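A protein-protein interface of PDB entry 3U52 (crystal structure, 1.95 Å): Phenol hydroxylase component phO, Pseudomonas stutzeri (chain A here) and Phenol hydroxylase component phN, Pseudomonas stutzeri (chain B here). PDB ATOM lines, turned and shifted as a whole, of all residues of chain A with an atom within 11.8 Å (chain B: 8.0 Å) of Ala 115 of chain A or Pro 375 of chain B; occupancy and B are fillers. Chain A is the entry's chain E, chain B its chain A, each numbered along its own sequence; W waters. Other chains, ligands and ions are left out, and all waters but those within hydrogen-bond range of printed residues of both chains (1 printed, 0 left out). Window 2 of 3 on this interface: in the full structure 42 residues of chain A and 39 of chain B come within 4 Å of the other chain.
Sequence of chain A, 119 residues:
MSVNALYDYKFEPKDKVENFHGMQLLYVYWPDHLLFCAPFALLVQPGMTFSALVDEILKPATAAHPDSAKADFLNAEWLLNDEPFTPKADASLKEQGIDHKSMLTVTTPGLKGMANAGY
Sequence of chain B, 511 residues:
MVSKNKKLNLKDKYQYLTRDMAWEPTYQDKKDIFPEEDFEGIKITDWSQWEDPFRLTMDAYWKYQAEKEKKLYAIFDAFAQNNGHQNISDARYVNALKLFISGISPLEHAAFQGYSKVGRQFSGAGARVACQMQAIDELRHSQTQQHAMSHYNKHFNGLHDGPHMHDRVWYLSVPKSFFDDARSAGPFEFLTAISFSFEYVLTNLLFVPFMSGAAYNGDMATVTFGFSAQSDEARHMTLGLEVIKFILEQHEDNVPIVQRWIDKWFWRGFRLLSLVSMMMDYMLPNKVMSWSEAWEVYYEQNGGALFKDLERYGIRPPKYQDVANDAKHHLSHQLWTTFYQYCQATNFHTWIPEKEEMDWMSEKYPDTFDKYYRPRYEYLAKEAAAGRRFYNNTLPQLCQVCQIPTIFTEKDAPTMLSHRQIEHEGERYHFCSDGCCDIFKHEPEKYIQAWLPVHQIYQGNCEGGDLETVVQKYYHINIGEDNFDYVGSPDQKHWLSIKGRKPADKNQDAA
N of Leu 34 of chain A is in hydrogen-bond range of OXT of Tyr 119 of chain A, 3.1 Å away. The guanidinium group (NE) of Arg 376 of chain B is in hydrogen-bond range of the backbone carbonyl oxygen (O) of Tyr 372 of chain B, at 3.4 Å. N of Leu 35 of chain A is in hydrogen-bond range of OXT of Tyr 119 of chain A, 2.8 Å away. O of Tyr 119 of chain A lies within hydrogen-bond range of NE2 of His 65 of chain A (2.8 Å). The chain-end carboxylate (O) of Tyr 119 of chain A lies within hydrogen-bond range of the backbone NH (N) of Met 114 of chain A, at 2.7 Å. N of Leu 34 of chain A is in hydrogen-bond range of O of Gly 118 of chain A.
Arg 376 of chain B touches Leu 34 of chain A. OH of Tyr 379 of chain B touches CD of Pro 66 of chain A, at 3.4 Å. Tyr 379 of chain B touches Met 114 of chain A. Pro 375 of chain B touches Ala 115 of chain A. Ala 117 of chain A touches Lys 371 of chain B. CD2 of Tyr 119 of chain A touches NE of Arg 376 of chain B, at 3.5 Å. Tyr 119 of chain A touches Leu 380 of chain B.
Lys 112 of chain A touches none of the printed residues of chain B. Of the printed residues of chain B, Met 114 of chain A touches Tyr 379 (3.0 Å). Ala 115 of chain A touches just one residue of chain B: Pro 375. No residue of chain A comes within 4 Å of Phe 369 of chain B. Of the printed residues of chain A, Lys 371 of chain B touches Ala 117 (3.5 Å). Pro 375 of chain B touches just one residue of chain A: Ala 115. Printed residues of chain A within 4 Å of Arg 376 of chain B: Leu 34 (3.8 Å) and Tyr 119 (3.5 Å). Ala 381 of chain B touches none of the printed residues of chain A. The nearest residue of chain B that does not touch Ala 115 of chain A is Lys 371 of chain B (4.6 Å). The nearest residue of chain A that does not touch Pro 375 of chain B is Ala 117 of chain A (4.5 Å). The nearest printed residue of chain B that does not touch Ala 117 of chain A is Tyr 372 of chain B (4.2 Å).
Along chain B the printed residues that touch a printed residue of chain A span positions 371 to 380. Printed residues of chain A that touch a printed residue of chain B: Leu 34, Pro 66, Met 114, Ala 115, Ala 117 and Tyr 119. Hydrophobic or aromatic side chains of chain A that line the printed part of chain B: Leu 34, Pro 66, Met 114, Ala 115, Ala 117 and Tyr 119. Among the printed residues, no Asp or Glu carboxylate lies within 4 Å of a Lys or Arg side-chain nitrogen of the other chain.
Water W1 lies within hydrogen-bond range of O of Ala 117 of chain A (2.7 Å), NH2 of Arg 376 of chain B (2.8 Å) and O of Tyr 372 of chain B (2.9 Å).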
ATOM      1  N   ASP A  32      17.792   1.592  17.621  1.00  0.00           N
ATOM      2  CA  ASP A  32      17.125   1.519  16.304  1.00  0.00           C
ATOM      3  C   ASP A  32      15.619   1.483  16.383  1.00  0.00           C
ATOM      4  O   ASP A  32      14.971   0.985  15.457  1.00  0.00           O
ATOM      5  CB  ASP A  32      17.665   0.335  15.485  1.00  0.00           C
ATOM      6  CG  ASP A  32      19.127   0.510  15.149  1.00  0.00           C
ATOM      7  OD1 ASP A  32      19.511   1.621  14.688  1.00  0.00           O
ATOM      8  OD2 ASP A  32      19.889  -0.455  15.381  1.00  0.00           O
ATOM      9  N   HIS A  33      15.069   2.026  17.471  1.00  0.00           N
ATOM     10  CA  HIS A  33      13.623   2.059  17.684  1.00  0.00           C
ATOM     11  C   HIS A  33      13.166   3.438  18.172  1.00  0.00           C
ATOM     12  O   HIS A  33      12.527   3.574  19.233  1.00  0.00           O
ATOM     13  CB  HIS A  33      13.175   0.896  18.578  1.00  0.00           C
ATOM     14  CG  HIS A  33      13.369  -0.428  17.901  1.00  0.00           C
ATOM     15  ND1 HIS A  33      14.615  -1.016  17.786  1.00  0.00           N
ATOM     16  CD2 HIS A  33      12.527  -1.181  17.152  1.00  0.00           C
ATOM     17  CE1 HIS A  33      14.517  -2.113  17.045  1.00  0.00           C
ATOM     18  NE2 HIS A  33      13.258  -2.241  16.660  1.00  0.00           N
ATOM     19  N   LEU A  34      13.516   4.452  17.376  1.00  0.00           N
ATOM     20  CA  LEU A  34      13.405   5.863  17.808  1.00  0.00           C
ATOM     21  C   LEU A  34      11.966   6.319  17.771  1.00  0.00           C
ATOM     22  O   LEU A  34      11.664   7.466  18.117  1.00  0.00           O
ATOM     23  CB  LEU A  34      14.324   6.792  16.983  1.00  0.00           C
ATOM     24  CG  LEU A  34      15.818   6.539  17.269  1.00  0.00           C
ATOM     25  CD1 LEU A  34      16.657   7.169  16.199  1.00  0.00           C
ATOM     26  CD2 LEU A  34      16.119   7.040  18.653  1.00  0.00           C
ATOM     27  N   LEU A  35      11.053   5.416  17.388  1.00  0.00           N
ATOM     28  CA  LEU A  35       9.638   5.652  17.648  1.00  0.00           C
ATOM     29  C   LEU A  35       9.414   6.137  19.096  1.00  0.00           C
ATOM     30  O   LEU A  35       8.560   7.032  19.345  1.00  0.00           O
ATOM     31  CB  LEU A  35       8.771   4.410  17.310  1.00  0.00           C
ATOM     32  CG  LEU A  35       7.255   4.415  17.654  1.00  0.00           C
ATOM     33  CD1 LEU A  35       6.373   5.411  16.887  1.00  0.00           C
ATOM     34  CD2 LEU A  35       6.618   3.014  17.552  1.00  0.00           C
ATOM     35  N   HIS A  65       5.427  -0.400  18.762  1.00  0.00           N
ATOM     36  CA  HIS A  65       6.314  -0.591  17.618  1.00  0.00           C
ATOM     37  C   HIS A  65       6.006  -1.911  16.950  1.00  0.00           C
ATOM     38  O   HIS A  65       5.914  -2.916  17.642  1.00  0.00           O
ATOM     39  CB  HIS A  65       7.802  -0.577  18.041  1.00  0.00           C
ATOM     40  CG  HIS A  65       8.728  -0.367  16.891  1.00  0.00           C
ATOM     41  ND1 HIS A  65       8.986  -1.348  15.967  1.00  0.00           N
ATOM     42  CD2 HIS A  65       9.385   0.738  16.461  1.00  0.00           C
ATOM     43  CE1 HIS A  65       9.803  -0.876  15.039  1.00  0.00           C
ATOM     44  NE2 HIS A  65      10.030   0.397  15.294  1.00  0.00           N
ATOM     45  N   PRO A  66       5.914  -1.931  15.616  1.00  0.00           N
ATOM     46  CA  PRO A  66       5.779  -3.164  14.819  1.00  0.00           C
ATOM     47  C   PRO A  66       6.766  -4.290  15.132  1.00  0.00           C
ATOM     48  O   PRO A  66       6.365  -5.442  15.108  1.00  0.00           O
ATOM     49  CB  PRO A  66       6.023  -2.673  13.396  1.00  0.00           C
ATOM     50  CG  PRO A  66       5.461  -1.342  13.410  1.00  0.00           C
ATOM     51  CD  PRO A  66       5.908  -0.752  14.725  1.00  0.00           C
ATOM     52  N   ASP A  67       8.025  -3.979  15.432  1.00  0.00           N
ATOM     53  CA  ASP A  67       9.000  -5.011  15.834  1.00  0.00           C
ATOM     54  C   ASP A  67       8.746  -5.715  17.199  1.00  0.00           C
ATOM     55  O   ASP A  67       9.346  -6.773  17.466  1.00  0.00           O
ATOM     56  CB  ASP A  67      10.413  -4.433  15.907  1.00  0.00           C
ATOM     57  CG  ASP A  67      10.998  -4.103  14.569  1.00  0.00           C
ATOM     58  OD1 ASP A  67      10.359  -4.385  13.535  1.00  0.00           O
ATOM     59  OD2 ASP A  67      12.121  -3.551  14.567  1.00  0.00           O
ATOM     60  N   LYS A  70       7.679  -9.393  17.395  1.00  0.00           N
ATOM     61  CA  LYS A  70       8.693 -10.328  16.871  1.00  0.00           C
ATOM     62  C   LYS A  70       9.925 -10.509  17.780  1.00  0.00           C
ATOM     63  O   LYS A  70      10.750 -11.381  17.532  1.00  0.00           O
ATOM     64  CB  LYS A  70       9.138  -9.895  15.464  1.00  0.00           C
ATOM     65  CG  LYS A  70       8.003  -9.384  14.550  1.00  0.00           C
ATOM     66  CD  LYS A  70       8.527  -8.949  13.193  1.00  0.00           C
ATOM     67  CE  LYS A  70       7.421  -8.315  12.341  1.00  0.00           C
ATOM     68  NZ  LYS A  70       7.956  -7.745  11.058  1.00  0.00           N
ATOM     69  N   GLY A 110      18.309  -8.232  13.604  1.00  0.00           N
ATOM     70  CA  GLY A 110      17.239  -8.523  12.651  1.00  0.00           C
ATOM     71  C   GLY A 110      16.032  -7.622  12.806  1.00  0.00           C
ATOM     72  O   GLY A 110      15.154  -7.574  11.918  1.00  0.00           O
ATOM     73  N   LEU A 111      15.967  -6.904  13.925  1.00  0.00           N
ATOM     74  CA  LEU A 111      14.872  -5.960  14.123  1.00  0.00           C
ATOM     75  C   LEU A 111      15.532  -4.608  14.316  1.00  0.00           C
ATOM     76  O   LEU A 111      15.994  -4.281  15.409  1.00  0.00           O
ATOM     77  CB  LEU A 111      13.994  -6.362  15.312  1.00  0.00           C
ATOM     78  CG  LEU A 111      13.371  -7.763  15.242  1.00  0.00           C
ATOM     79  CD1 LEU A 111      12.650  -8.055  16.497  1.00  0.00           C
ATOM     80  CD2 LEU A 111      12.457  -7.956  14.032  1.00  0.00           C
ATOM     81  N   LYS A 112      15.612  -3.848  13.222  1.00  0.00           N
ATOM     82  CA  LYS A 112      16.398  -2.638  13.207  1.00  0.00           C
ATOM     83  C   LYS A 112      15.534  -1.413  12.919  1.00  0.00           C
ATOM     84  O   LYS A 112      16.024  -0.388  12.516  1.00  0.00           O
ATOM     85  CB  LYS A 112      17.513  -2.751  12.186  1.00  0.00           C
ATOM     86  CG  LYS A 112      16.984  -2.914  10.791  1.00  0.00           C
ATOM     87  CD  LYS A 112      18.091  -2.866   9.748  1.00  0.00           C
ATOM     88  CE  LYS A 112      17.619  -3.504   8.467  1.00  0.00           C
ATOM     89  NZ  LYS A 112      16.435  -2.793   7.927  1.00  0.00           N
ATOM     90  N   GLY A 113      14.243  -1.522  13.105  1.00  0.00           N
ATOM     91  CA  GLY A 113      13.428  -0.343  13.018  1.00  0.00           C
ATOM     92  C   GLY A 113      12.929  -0.156  11.592  1.00  0.00           C
ATOM     93  O   GLY A 113      13.238  -0.947  10.671  1.00  0.00           O
ATOM     94  N   MET A 114      12.113   0.860  11.427  1.00  0.00           N
ATOM     95  CA  MET A 114      11.460   1.090  10.167  1.00  0.00           C
ATOM     96  C   MET A 114      12.286   1.978   9.269  1.00  0.00           C
ATOM     97  O   MET A 114      13.047   2.850   9.733  1.00  0.00           O
ATOM     98  CB  MET A 114      10.074   1.703  10.375  1.00  0.00           C
ATOM     99  CG  MET A 114       9.126   0.826  11.206  1.00  0.00           C
ATOM    100  SD  MET A 114       7.698   1.831  11.668  1.00  0.00           S
ATOM    101  CE  MET A 114       6.779   1.512  10.146  1.00  0.00           C
ATOM    102  N   ALA A 115      12.152   1.681   7.973  1.00  0.00           N
ATOM    103  CA  ALA A 115      12.465   2.566   6.873  1.00  0.00           C
ATOM    104  C   ALA A 115      13.950   2.895   6.711  1.00  0.00           C
ATOM    105  O   ALA A 115      14.303   3.963   6.205  1.00  0.00           O
ATOM    106  CB  ALA A 115      11.607   3.865   6.994  1.00  0.00           C
ATOM    107  N   ASN A 116      14.825   1.996   7.138  1.00  0.00           N
ATOM    108  CA  ASN A 116      16.246   2.296   7.163  1.00  0.00           C
ATOM    109  C   ASN A 116      16.614   3.565   7.947  1.00  0.00           C
ATOM    110  O   ASN A 116      17.649   4.203   7.681  1.00  0.00           O
ATOM    111  CB  ASN A 116      16.806   2.339   5.724  1.00  0.00           C
ATOM    112  CG  ASN A 116      17.016   0.957   5.160  1.00  0.00           C
ATOM    113  OD1 ASN A 116      16.247   0.483   4.307  1.00  0.00           O
ATOM    114  ND2 ASN A 116      18.034   0.271   5.671  1.00  0.00           N
ATOM    115  N   ALA A 117      15.758   3.926   8.901  1.00  0.00           N
ATOM    116  CA  ALA A 117      15.870   5.177   9.648  1.00  0.00           C
ATOM    117  C   ALA A 117      15.935   4.928  11.172  1.00  0.00           C
ATOM    118  O   ALA A 117      15.888   5.877  11.957  1.00  0.00           O
ATOM    119  CB  ALA A 117      14.685   6.121   9.282  1.00  0.00           C
ATOM    120  N   GLY A 118      16.029   3.655  11.580  1.00  0.00           N
ATOM    121  CA  GLY A 118      16.152   3.244  13.012  1.00  0.00           C
ATOM    122  C   GLY A 118      14.967   3.718  13.860  1.00  0.00           C
ATOM    123  O   GLY A 118      15.131   4.074  15.028  1.00  0.00           O
ATOM    124  N   TYR A 119      13.789   3.740  13.241  1.00  0.00           N
ATOM    125  CA  TYR A 119      12.600   4.300  13.828  1.00  0.00           C
ATOM    126  C   TYR A 119      11.708   3.180  14.357  1.00  0.00           C
ATOM    127  O   TYR A 119      11.371   2.182  13.649  1.00  0.00           O
ATOM    128  CB  TYR A 119      11.858   5.155  12.819  1.00  0.00           C
ATOM    129  CG  TYR A 119      10.737   5.969  13.419  1.00  0.00           C
ATOM    130  CD1 TYR A 119       9.402   5.751  13.011  1.00  0.00           C
ATOM    131  CD2 TYR A 119      11.003   6.960  14.396  1.00  0.00           C
ATOM    132  CE1 TYR A 119       8.339   6.524  13.558  1.00  0.00           C
ATOM    133  CE2 TYR A 119       9.923   7.742  14.973  1.00  0.00           C
ATOM    134  CZ  TYR A 119       8.602   7.497  14.531  1.00  0.00           C
ATOM    135  OH  TYR A 119       7.550   8.262  15.054  1.00  0.00           O
ATOM    136  OXT TYR A 119      11.360   3.243  15.575  1.00  0.00           O
ATOM    137  N   MET B 358       5.889  19.621   4.757  1.00  0.00           N
ATOM    138  CA  MET B 358       6.894  18.606   4.555  1.00  0.00           C
ATOM    139  C   MET B 358       7.772  18.808   3.331  1.00  0.00           C
ATOM    140  O   MET B 358       8.990  18.547   3.400  1.00  0.00           O
ATOM    141  CB  MET B 358       6.254  17.234   4.564  1.00  0.00           C
ATOM    142  CG  MET B 358       6.084  16.709   6.024  1.00  0.00           C
ATOM    143  SD  MET B 358       5.263  15.181   6.224  1.00  0.00           S
ATOM    144  CE  MET B 358       6.345  13.962   5.487  1.00  0.00           C
ATOM    145  N   THR B 368      18.865  15.415   5.476  1.00  0.00           N
ATOM    146  CA  THR B 368      18.305  14.693   6.652  1.00  0.00           C
ATOM    147  C   THR B 368      16.787  14.423   6.671  1.00  0.00           C
ATOM    148  O   THR B 368      16.363  13.386   7.189  1.00  0.00           O
ATOM    149  CB  THR B 368      18.627  15.430   7.962  1.00  0.00           C
ATOM    150  OG1 THR B 368      18.100  16.772   7.900  1.00  0.00           O
ATOM    151  CG2 THR B 368      20.158  15.493   8.199  1.00  0.00           C
ATOM    152  N   PHE B 369      15.964  15.320   6.123  1.00  0.00           N
ATOM    153  CA  PHE B 369      14.544  15.181   6.352  1.00  0.00           C
ATOM    154  C   PHE B 369      13.948  13.941   5.695  1.00  0.00           C
ATOM    155  O   PHE B 369      13.232  13.178   6.355  1.00  0.00           O
ATOM    156  CB  PHE B 369      13.750  16.412   5.959  1.00  0.00           C
ATOM    157  CG  PHE B 369      12.295  16.334   6.386  1.00  0.00           C
ATOM    158  CD1 PHE B 369      11.920  16.587   7.711  1.00  0.00           C
ATOM    159  CD2 PHE B 369      11.304  16.002   5.456  1.00  0.00           C
ATOM    160  CE1 PHE B 369      10.574  16.496   8.090  1.00  0.00           C
ATOM    161  CE2 PHE B 369       9.945  15.922   5.826  1.00  0.00           C
ATOM    162  CZ  PHE B 369       9.597  16.180   7.155  1.00  0.00           C
ATOM    163  N   ASP B 370      14.233  13.734   4.411  1.00  0.00           N
ATOM    164  CA  ASP B 370      13.656  12.590   3.700  1.00  0.00           C
ATOM    165  C   ASP B 370      14.195  11.275   4.194  1.00  0.00           C
ATOM    166  O   ASP B 370      13.463  10.284   4.249  1.00  0.00           O
ATOM    167  CB  ASP B 370      13.838  12.731   2.188  1.00  0.00           C
ATOM    168  CG  ASP B 370      12.947  13.820   1.604  1.00  0.00           C
ATOM    169  OD1 ASP B 370      11.988  14.249   2.276  1.00  0.00           O
ATOM    170  OD2 ASP B 370      13.186  14.249   0.462  1.00  0.00           O
ATOM    171  N   LYS B 371      15.468  11.277   4.589  1.00  0.00           N
ATOM    172  CA  LYS B 371      16.111  10.063   5.086  1.00  0.00           C
ATOM    173  C   LYS B 371      15.601   9.644   6.469  1.00  0.00           C
ATOM    174  O   LYS B 371      15.260   8.469   6.705  1.00  0.00           O
ATOM    175  CB  LYS B 371      17.623  10.266   5.164  1.00  0.00           C
ATOM    176  CG  LYS B 371      18.401   8.954   5.360  1.00  0.00           C
ATOM    177  CD  LYS B 371      19.888   9.121   5.044  1.00  0.00           C
ATOM    178  CE  LYS B 371      20.141   9.774   3.651  1.00  0.00           C
ATOM    179  NZ  LYS B 371      21.612   9.895   3.320  1.00  0.00           N
ATOM    180  N   TYR B 372      15.569  10.594   7.406  1.00  0.00           N
ATOM    181  CA  TYR B 372      15.329  10.266   8.821  1.00  0.00           C
ATOM    182  C   TYR B 372      13.973  10.666   9.328  1.00  0.00           C
ATOM    183  O   TYR B 372      13.490  10.036  10.259  1.00  0.00           O
ATOM    184  CB  TYR B 372      16.401  10.880   9.748  1.00  0.00           C
ATOM    185  CG  TYR B 372      17.809  10.472   9.429  1.00  0.00           C
ATOM    186  CD1 TYR B 372      18.708  11.376   8.862  1.00  0.00           C
ATOM    187  CD2 TYR B 372      18.232   9.187   9.660  1.00  0.00           C
ATOM    188  CE1 TYR B 372      20.025  11.002   8.563  1.00  0.00           C
ATOM    189  CE2 TYR B 372      19.522   8.783   9.359  1.00  0.00           C
ATOM    190  CZ  TYR B 372      20.415   9.694   8.800  1.00  0.00           C
ATOM    191  OH  TYR B 372      21.693   9.239   8.522  1.00  0.00           O
ATOM    192  N   TYR B 373      13.346  11.704   8.762  1.00  0.00           N
ATOM    193  CA  TYR B 373      12.146  12.256   9.400  1.00  0.00           C
ATOM    194  C   TYR B 373      10.825  12.067   8.678  1.00  0.00           C
ATOM    195  O   TYR B 373       9.828  11.700   9.305  1.00  0.00           O
ATOM    196  CB  TYR B 373      12.406  13.701   9.936  1.00  0.00           C
ATOM    197  CG  TYR B 373      13.650  13.728  10.821  1.00  0.00           C
ATOM    198  CD1 TYR B 373      14.822  14.351  10.418  1.00  0.00           C
ATOM    199  CD2 TYR B 373      13.652  13.070  12.067  1.00  0.00           C
ATOM    200  CE1 TYR B 373      15.980  14.312  11.202  1.00  0.00           C
ATOM    201  CE2 TYR B 373      14.799  13.051  12.868  1.00  0.00           C
ATOM    202  CZ  TYR B 373      15.951  13.662  12.441  1.00  0.00           C
ATOM    203  OH  TYR B 373      17.050  13.593  13.283  1.00  0.00           O
ATOM    204  N   ARG B 374      10.807  12.275   7.366  1.00  0.00           N
ATOM    205  CA  ARG B 374       9.619  12.034   6.542  1.00  0.00           C
ATOM    206  C   ARG B 374       8.973  10.642   6.804  1.00  0.00           C
ATOM    207  O   ARG B 374       7.774  10.570   6.979  1.00  0.00           O
ATOM    208  CB  ARG B 374       9.951  12.251   5.052  1.00  0.00           C
ATOM    209  CG  ARG B 374       8.739  12.153   4.089  1.00  0.00           C
ATOM    210  CD  ARG B 374       9.198  12.416   2.661  1.00  0.00           C
ATOM    211  NE  ARG B 374       9.315  13.839   2.371  1.00  0.00           N
ATOM    212  CZ  ARG B 374       8.272  14.622   2.074  1.00  0.00           C
ATOM    213  NH1 ARG B 374       7.050  14.114   2.061  1.00  0.00           N
ATOM    214  NH2 ARG B 374       8.446  15.922   1.795  1.00  0.00           N
ATOM    215  N   PRO B 375       9.774   9.549   6.859  1.00  0.00           N
ATOM    216  CA  PRO B 375       9.182   8.228   7.123  1.00  0.00           C
ATOM    217  C   PRO B 375       8.451   8.132   8.483  1.00  0.00           C
ATOM    218  O   PRO B 375       7.505   7.389   8.607  1.00  0.00           O
ATOM    219  CB  PRO B 375      10.372   7.274   7.122  1.00  0.00           C
ATOM    220  CG  PRO B 375      11.579   8.070   6.729  1.00  0.00           C
ATOM    221  CD  PRO B 375      11.232   9.491   6.599  1.00  0.00           C
ATOM    222  N   ARG B 376       8.883   8.920   9.477  1.00  0.00           N
ATOM    223  CA  ARG B 376       8.204   8.954  10.766  1.00  0.00           C
ATOM    224  C   ARG B 376       6.799   9.456  10.575  1.00  0.00           C
ATOM    225  O   ARG B 376       5.873   8.859  11.118  1.00  0.00           O
ATOM    226  CB  ARG B 376       8.891   9.897  11.738  1.00  0.00           C
ATOM    227  CG  ARG B 376      10.329   9.561  11.991  1.00  0.00           C
ATOM    228  CD  ARG B 376      10.922  10.516  13.095  1.00  0.00           C
ATOM    229  NE  ARG B 376      12.271  10.021  13.388  1.00  0.00           N
ATOM    230  CZ  ARG B 376      12.971  10.322  14.470  1.00  0.00           C
ATOM    231  NH1 ARG B 376      12.462  11.164  15.397  1.00  0.00           N
ATOM    232  NH2 ARG B 376      14.184   9.789  14.605  1.00  0.00           N
ATOM    233  N   TYR B 377       6.647  10.578   9.863  1.00  0.00           N
ATOM    234  CA  TYR B 377       5.313  11.175   9.639  1.00  0.00           C
ATOM    235  C   TYR B 377       4.443  10.262   8.740  1.00  0.00           C
ATOM    236  O   TYR B 377       3.245  10.142   8.957  1.00  0.00           O
ATOM    237  CB  TYR B 377       5.436  12.611   9.098  1.00  0.00           C
ATOM    238  CG  TYR B 377       6.271  13.517  10.042  1.00  0.00           C
ATOM    239  CD1 TYR B 377       5.877  13.729  11.372  1.00  0.00           C
ATOM    240  CD2 TYR B 377       7.452  14.132   9.604  1.00  0.00           C
ATOM    241  CE1 TYR B 377       6.670  14.528  12.256  1.00  0.00           C
ATOM    242  CE2 TYR B 377       8.239  14.922  10.462  1.00  0.00           C
ATOM    243  CZ  TYR B 377       7.842  15.102  11.778  1.00  0.00           C
ATOM    244  OH  TYR B 377       8.607  15.876  12.610  1.00  0.00           O
ATOM    245  N   GLU B 378       5.062   9.574   7.783  1.00  0.00           N
ATOM    246  CA  GLU B 378       4.313   8.592   6.982  1.00  0.00           C
ATOM    247  C   GLU B 378       3.675   7.509   7.885  1.00  0.00           C
ATOM    248  O   GLU B 378       2.452   7.269   7.816  1.00  0.00           O
ATOM    249  CB  GLU B 378       5.195   8.011   5.896  1.00  0.00           C
ATOM    250  CG  GLU B 378       5.690   9.078   4.930  1.00  0.00           C
ATOM    251  CD  GLU B 378       6.574   8.516   3.827  1.00  0.00           C
ATOM    252  OE1 GLU B 378       6.816   9.232   2.815  1.00  0.00           O
ATOM    253  OE2 GLU B 378       7.027   7.361   3.959  1.00  0.00           O
ATOM    254  N   TYR B 379       4.502   6.888   8.739  1.00  0.00           N
ATOM    255  CA  TYR B 379       4.043   5.895   9.712  1.00  0.00           C
ATOM    256  C   TYR B 379       3.028   6.442  10.720  1.00  0.00           C
ATOM    257  O   TYR B 379       1.996   5.811  10.965  1.00  0.00           O
ATOM    258  CB  TYR B 379       5.238   5.252  10.459  1.00  0.00           C
ATOM    259  CG  TYR B 379       4.793   4.246  11.516  1.00  0.00           C
ATOM    260  CD1 TYR B 379       4.354   2.948  11.155  1.00  0.00           C
ATOM    261  CD2 TYR B 379       4.759   4.600  12.847  1.00  0.00           C
ATOM    262  CE1 TYR B 379       3.902   2.020  12.129  1.00  0.00           C
ATOM    263  CE2 TYR B 379       4.296   3.688  13.833  1.00  0.00           C
ATOM    264  CZ  TYR B 379       3.888   2.405  13.451  1.00  0.00           C
ATOM    265  OH  TYR B 379       3.434   1.526  14.393  1.00  0.00           O
ATOM    266  N   LEU B 380       3.313   7.614  11.309  1.00  0.00           N
ATOM    267  CA  LEU B 380       2.412   8.134  12.343  1.00  0.00           C
ATOM    268  C   LEU B 380       1.052   8.505  11.743  1.00  0.00           C
ATOM    269  O   LEU B 380       0.027   8.331  12.387  1.00  0.00           O
ATOM    270  CB  LEU B 380       3.026   9.355  13.033  1.00  0.00           C
ATOM    271  CG  LEU B 380       4.267   9.069  13.850  1.00  0.00           C
ATOM    272  CD1 LEU B 380       4.923  10.414  14.224  1.00  0.00           C
ATOM    273  CD2 LEU B 380       3.902   8.212  15.069  1.00  0.00           C
ATOM    274  N   ALA B 381       1.046   8.964  10.490  1.00  0.00           N
ATOM    275  CA  ALA B 381      -0.238   9.285   9.840  1.00  0.00           C
ATOM    276  C   ALA B 381      -1.071   8.026   9.490  1.00  0.00           C
ATOM    277  O   ALA B 381      -2.291   8.018   9.641  1.00  0.00           O
ATOM    278  CB  ALA B 381      -0.010  10.147   8.618  1.00  0.00           C
ATOM    279  N   LYS B 382      -0.413   6.976   9.047  1.00  0.00           N
ATOM    280  CA  LYS B 382      -1.105   5.716   8.801  1.00  0.00           C
ATOM    281  C   LYS B 382      -1.698   5.189  10.111  1.00  0.00           C
ATOM    282  O   LYS B 382      -2.875   4.781  10.169  1.00  0.00           O
ATOM    283  CB  LYS B 382      -0.102   4.705   8.288  1.00  0.00           C
ATOM    284  CG  LYS B 382       0.211   4.799   6.820  1.00  0.00           C
ATOM    285  CD  LYS B 382       1.534   4.053   6.538  1.00  0.00           C
ATOM    286  CE  LYS B 382       2.062   3.269   7.785  1.00  0.00           C
ATOM    287  NZ  LYS B 382       1.223   2.096   8.322  1.00  0.00           N
HETATM  288  O   HOH W   1      14.669   8.317  12.236  1.00  0.00           O
